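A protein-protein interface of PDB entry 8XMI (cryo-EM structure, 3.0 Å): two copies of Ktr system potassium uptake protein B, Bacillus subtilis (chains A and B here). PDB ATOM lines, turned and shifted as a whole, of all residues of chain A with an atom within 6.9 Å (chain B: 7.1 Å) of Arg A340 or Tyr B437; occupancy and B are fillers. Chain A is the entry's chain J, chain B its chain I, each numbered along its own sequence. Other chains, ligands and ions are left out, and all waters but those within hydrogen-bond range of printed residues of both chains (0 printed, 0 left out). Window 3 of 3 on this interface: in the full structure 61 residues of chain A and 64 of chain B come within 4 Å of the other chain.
The backbone carbonyl oxygen (O) of Pro B438 sits at hydrogen-bond distance from the backbone NH (N) of Ser A342 (2.8 Å). N of Gly B440 sits at hydrogen-bond distance from O of Ser A342 (2.8 Å).
The side-chain carboxylate of Glu A335 lies within hydrogen-bond range of the side-chain hydroxyl of Ser A342.
Among the printed residues, merely in contact across the chains: Arg A341 with Pro B438 (3.3 Å), Ser A342 with Asp B439 (3.3 Å), Ser A342 with Tyr B437 (3.3 Å), Glu A335 with Arg B436 (3.4 Å), Glu A335 with Tyr B437 (3.5 Å), Arg A340 with Tyr B437 (3.5 Å), Val A337 with Tyr B437 (3.6 Å), Leu A226 with Gly B440 (3.8 Å), Arg A341 with Asp B439 (3.97 Å) and Arg A341 with Gly B440 (3.99 Å).
Printed residues of chain B within 4 Å of Glu A335: Arg B436 (3.4 Å) and Tyr B437 (3.5 Å). Of chain B, only Tyr B437 (3.5 Å) comes within 4 Å of Arg A340. Of the printed residues of chain B, Ser A342 touches Tyr B437 (3.3 Å), Pro B438 (2.8 Å), Asp B439 (3.3 Å) and Gly B440 (2.8 Å). Ile A343 touches none of the printed residues of chain B. Of the printed residues of chain A, Arg B436 touches Glu A335. Tyr B437 touches just these residues of chain A: Glu A335, Val A337, Arg A340 and Ser A342. Of the printed residues of chain A, Pro B438 touches Arg A341 (3.3 Å) and Ser A342 (2.8 Å). The nearest residue of chain A that does not touch Tyr B437 is Arg A341 (4.2 Å). The nearest printed residue of chain B that does not touch Leu A226 is Asp B439 (5.9 Å).
Of the 10 printed residues of chain A, 6 touch a printed residue of chain B. Hydrophobic or aromatic side chains of chain A that line the printed part of chain B: Leu A226 and Val A337. Along chain A the printed residues that touch a printed residue of chain B span positions 226 to 342. Of the 6 printed residues of chain B, 5 touch a printed residue of chain A. Hydrophobic or aromatic side chains of chain B within 4 Å of the printed part of chain A: Tyr B437 and Pro B438. Among the printed residues, no Asp or Glu carboxylate lies within 4 Å of a Lys or Arg side-chain nitrogen of the other chain.
No position is printed for both chains. Of the 12 pairs that touch across the chains among the printed residues, none has its exchanged pair printed and touching as well.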
ATOM      1  N   LEU A 226     -14.752   2.550   5.406  1.00  0.00           N
ATOM      2  CA  LEU A 226     -15.777   1.568   5.735  1.00  0.00           C
ATOM      3  C   LEU A 226     -17.149   2.028   5.261  1.00  0.00           C
ATOM      4  O   LEU A 226     -17.936   1.225   4.750  1.00  0.00           O
ATOM      5  CB  LEU A 226     -15.786   1.302   7.239  1.00  0.00           C
ATOM      6  CG  LEU A 226     -16.834   0.311   7.742  1.00  0.00           C
ATOM      7  CD1 LEU A 226     -16.685  -1.019   7.037  1.00  0.00           C
ATOM      8  CD2 LEU A 226     -16.727   0.134   9.239  1.00  0.00           C
ATOM      9  N   GLU A 335     -18.562  -8.384  19.502  1.00  0.00           N
ATOM     10  CA  GLU A 335     -18.444  -7.080  18.869  1.00  0.00           C
ATOM     11  C   GLU A 335     -18.963  -7.150  17.441  1.00  0.00           C
ATOM     12  O   GLU A 335     -19.024  -8.219  16.830  1.00  0.00           O
ATOM     13  CB  GLU A 335     -16.998  -6.575  18.883  1.00  0.00           C
ATOM     14  CG  GLU A 335     -16.028  -7.443  18.107  1.00  0.00           C
ATOM     15  CD  GLU A 335     -14.724  -6.732  17.819  1.00  0.00           C
ATOM     16  OE1 GLU A 335     -14.464  -5.686  18.450  1.00  0.00           O
ATOM     17  OE2 GLU A 335     -13.964  -7.211  16.954  1.00  0.00           O
ATOM     18  N   THR A 336     -19.324  -5.982  16.916  1.00  0.00           N
ATOM     19  CA  THR A 336     -19.861  -5.853  15.569  1.00  0.00           C
ATOM     20  C   THR A 336     -18.714  -5.597  14.601  1.00  0.00           C
ATOM     21  O   THR A 336     -17.999  -4.599  14.734  1.00  0.00           O
ATOM     22  CB  THR A 336     -20.878  -4.717  15.503  1.00  0.00           C
ATOM     23  OG1 THR A 336     -21.833  -4.868  16.557  1.00  0.00           O
ATOM     24  CG2 THR A 336     -21.601  -4.720  14.168  1.00  0.00           C
ATOM     25  N   VAL A 337     -18.540  -6.490  13.633  1.00  0.00           N
ATOM     26  CA  VAL A 337     -17.445  -6.417  12.674  1.00  0.00           C
ATOM     27  C   VAL A 337     -18.033  -6.443  11.272  1.00  0.00           C
ATOM     28  O   VAL A 337     -18.655  -7.436  10.874  1.00  0.00           O
ATOM     29  CB  VAL A 337     -16.443  -7.566  12.866  1.00  0.00           C
ATOM     30  CG1 VAL A 337     -15.414  -7.565  11.758  1.00  0.00           C
ATOM     31  CG2 VAL A 337     -15.765  -7.456  14.211  1.00  0.00           C
ATOM     32  N   ILE A 338     -17.839  -5.358  10.527  1.00  0.00           N
ATOM     33  CA  ILE A 338     -18.188  -5.297   9.113  1.00  0.00           C
ATOM     34  C   ILE A 338     -16.937  -4.917   8.341  1.00  0.00           C
ATOM     35  O   ILE A 338     -16.282  -3.924   8.674  1.00  0.00           O
ATOM     36  CB  ILE A 338     -19.318  -4.288   8.827  1.00  0.00           C
ATOM     37  CG1 ILE A 338     -20.326  -4.256   9.974  1.00  0.00           C
ATOM     38  CG2 ILE A 338     -20.026  -4.652   7.537  1.00  0.00           C
ATOM     39  CD1 ILE A 338     -21.580  -3.478   9.667  1.00  0.00           C
ATOM     40  N   PHE A 339     -16.616  -5.701   7.308  1.00  0.00           N
ATOM     41  CA  PHE A 339     -15.434  -5.488   6.468  1.00  0.00           C
ATOM     42  C   PHE A 339     -14.157  -5.430   7.302  1.00  0.00           C
ATOM     43  O   PHE A 339     -13.291  -4.579   7.087  1.00  0.00           O
ATOM     44  CB  PHE A 339     -15.575  -4.229   5.610  1.00  0.00           C
ATOM     45  CG  PHE A 339     -16.518  -4.382   4.456  1.00  0.00           C
ATOM     46  CD1 PHE A 339     -16.095  -4.959   3.272  1.00  0.00           C
ATOM     47  CD2 PHE A 339     -17.822  -3.937   4.548  1.00  0.00           C
ATOM     48  CE1 PHE A 339     -16.959  -5.096   2.210  1.00  0.00           C
ATOM     49  CE2 PHE A 339     -18.689  -4.074   3.491  1.00  0.00           C
ATOM     50  CZ  PHE A 339     -18.258  -4.653   2.319  1.00  0.00           C
ATOM     51  N   ARG A 340     -14.058  -6.344   8.273  1.00  0.00           N
ATOM     52  CA  ARG A 340     -12.886  -6.493   9.140  1.00  0.00           C
ATOM     53  C   ARG A 340     -12.583  -5.216   9.922  1.00  0.00           C
ATOM     54  O   ARG A 340     -11.425  -4.874  10.158  1.00  0.00           O
ATOM     55  CB  ARG A 340     -11.665  -6.948   8.340  1.00  0.00           C
ATOM     56  CG  ARG A 340     -11.820  -8.331   7.741  1.00  0.00           C
ATOM     57  CD  ARG A 340     -10.643  -8.695   6.857  1.00  0.00           C
ATOM     58  NE  ARG A 340     -10.709 -10.087   6.429  1.00  0.00           N
ATOM     59  CZ  ARG A 340      -9.814 -10.675   5.649  1.00  0.00           C
ATOM     60  NH1 ARG A 340      -8.770 -10.014   5.175  1.00  0.00           N
ATOM     61  NH2 ARG A 340      -9.968 -11.959   5.337  1.00  0.00           N
ATOM     62  N   ARG A 341     -13.632  -4.509  10.330  1.00  0.00           N
ATOM     63  CA  ARG A 341     -13.508  -3.309  11.145  1.00  0.00           C
ATOM     64  C   ARG A 341     -14.527  -3.374  12.267  1.00  0.00           C
ATOM     65  O   ARG A 341     -15.704  -3.643  12.021  1.00  0.00           O
ATOM     66  CB  ARG A 341     -13.733  -2.041  10.319  1.00  0.00           C
ATOM     67  CG  ARG A 341     -12.596  -1.665   9.390  1.00  0.00           C
ATOM     68  CD  ARG A 341     -11.369  -1.229  10.161  1.00  0.00           C
ATOM     69  NE  ARG A 341     -10.501  -0.376   9.362  1.00  0.00           N
ATOM     70  CZ  ARG A 341      -9.595  -0.823   8.505  1.00  0.00           C
ATOM     71  NH1 ARG A 341      -9.410  -2.117   8.306  1.00  0.00           N
ATOM     72  NH2 ARG A 341      -8.856   0.052   7.829  1.00  0.00           N
ATOM     73  N   SER A 342     -14.079  -3.126  13.490  1.00  0.00           N
ATOM     74  CA  SER A 342     -14.993  -3.070  14.618  1.00  0.00           C
ATOM     75  C   SER A 342     -15.796  -1.779  14.583  1.00  0.00           C
ATOM     76  O   SER A 342     -15.291  -0.715  14.222  1.00  0.00           O
ATOM     77  CB  SER A 342     -14.224  -3.171  15.931  1.00  0.00           C
ATOM     78  OG  SER A 342     -15.074  -2.949  17.039  1.00  0.00           O
ATOM     79  N   ILE A 343     -17.065  -1.876  14.965  1.00  0.00           N
ATOM     80  CA  ILE A 343     -17.964  -0.730  15.008  1.00  0.00           C
ATOM     81  C   ILE A 343     -18.309  -0.453  16.462  1.00  0.00           C
ATOM     82  O   ILE A 343     -18.823  -1.331  17.164  1.00  0.00           O
ATOM     83  CB  ILE A 343     -19.223  -0.972  14.162  1.00  0.00           C
ATOM     84  CG1 ILE A 343     -18.840  -1.047  12.683  1.00  0.00           C
ATOM     85  CG2 ILE A 343     -20.235   0.121  14.398  1.00  0.00           C
ATOM     86  CD1 ILE A 343     -20.002  -0.967  11.743  1.00  0.00           C
ATOM     87  N   ILE B 435      -9.962 -12.412  19.396  1.00  0.00           N
ATOM     88  CA  ILE B 435      -9.327 -11.373  18.597  1.00  0.00           C
ATOM     89  C   ILE B 435     -10.281 -10.199  18.428  1.00  0.00           C
ATOM     90  O   ILE B 435     -11.506 -10.342  18.484  1.00  0.00           O
ATOM     91  CB  ILE B 435      -8.870 -11.939  17.239  1.00  0.00           C
ATOM     92  CG1 ILE B 435     -10.066 -12.223  16.333  1.00  0.00           C
ATOM     93  CG2 ILE B 435      -8.066 -13.203  17.442  1.00  0.00           C
ATOM     94  CD1 ILE B 435      -9.682 -12.794  14.992  1.00  0.00           C
ATOM     95  N   ARG B 436      -9.707  -9.017  18.235  1.00  0.00           N
ATOM     96  CA  ARG B 436     -10.459  -7.788  18.054  1.00  0.00           C
ATOM     97  C   ARG B 436      -9.984  -7.110  16.780  1.00  0.00           C
ATOM     98  O   ARG B 436      -8.997  -7.518  16.168  1.00  0.00           O
ATOM     99  CB  ARG B 436     -10.304  -6.857  19.261  1.00  0.00           C
ATOM    100  CG  ARG B 436     -10.898  -7.412  20.540  1.00  0.00           C
ATOM    101  CD  ARG B 436     -12.409  -7.529  20.431  1.00  0.00           C
ATOM    102  NE  ARG B 436     -13.013  -8.177  21.590  1.00  0.00           N
ATOM    103  CZ  ARG B 436     -13.515  -9.405  21.588  1.00  0.00           C
ATOM    104  NH1 ARG B 436     -13.513 -10.150  20.495  1.00  0.00           N
ATOM    105  NH2 ARG B 436     -14.037  -9.895  22.708  1.00  0.00           N
ATOM    106  N   TYR B 437     -10.696  -6.067  16.376  1.00  0.00           N
ATOM    107  CA  TYR B 437     -10.442  -5.423  15.099  1.00  0.00           C
ATOM    108  C   TYR B 437     -10.339  -3.917  15.266  1.00  0.00           C
ATOM    109  O   TYR B 437     -10.895  -3.356  16.215  1.00  0.00           O
ATOM    110  CB  TYR B 437     -11.556  -5.756  14.100  1.00  0.00           C
ATOM    111  CG  TYR B 437     -11.469  -7.147  13.534  1.00  0.00           C
ATOM    112  CD1 TYR B 437     -10.647  -7.424  12.458  1.00  0.00           C
ATOM    113  CD2 TYR B 437     -12.213  -8.181  14.072  1.00  0.00           C
ATOM    114  CE1 TYR B 437     -10.567  -8.688  11.936  1.00  0.00           C
ATOM    115  CE2 TYR B 437     -12.137  -9.452  13.555  1.00  0.00           C
ATOM    116  CZ  TYR B 437     -11.315  -9.699  12.488  1.00  0.00           C
ATOM    117  OH  TYR B 437     -11.238 -10.965  11.964  1.00  0.00           O
ATOM    118  N   PRO B 438      -9.615  -3.239  14.375  1.00  0.00           N
ATOM    119  CA  PRO B 438      -9.536  -1.778  14.451  1.00  0.00           C
ATOM    120  C   PRO B 438     -10.872  -1.123  14.148  1.00  0.00           C
ATOM    121  O   PRO B 438     -11.700  -1.656  13.407  1.00  0.00           O
ATOM    122  CB  PRO B 438      -8.490  -1.424  13.388  1.00  0.00           C
ATOM    123  CG  PRO B 438      -8.493  -2.573  12.464  1.00  0.00           C
ATOM    124  CD  PRO B 438      -8.746  -3.768  13.314  1.00  0.00           C
ATOM    125  N   ASP B 439     -11.072   0.050  14.737  1.00  0.00           N
ATOM    126  CA  ASP B 439     -12.343   0.747  14.625  1.00  0.00           C
ATOM    127  C   ASP B 439     -12.548   1.308  13.224  1.00  0.00           C
ATOM    128  O   ASP B 439     -11.634   1.874  12.622  1.00  0.00           O
ATOM    129  CB  ASP B 439     -12.410   1.876  15.647  1.00  0.00           C
ATOM    130  CG  ASP B 439     -11.951   1.440  17.017  1.00  0.00           C
ATOM    131  OD1 ASP B 439     -11.654   0.239  17.186  1.00  0.00           O
ATOM    132  OD2 ASP B 439     -11.883   2.296  17.924  1.00  0.00           O
ATOM    133  N   GLY B 440     -13.759   1.151  12.714  1.00  0.00           N
ATOM    134  CA  GLY B 440     -14.161   1.769  11.460  1.00  0.00           C
ATOM    135  C   GLY B 440     -15.294   2.745  11.705  1.00  0.00           C
ATOM    136  O   GLY B 440     -16.204   2.460  12.485  1.00  0.00           O
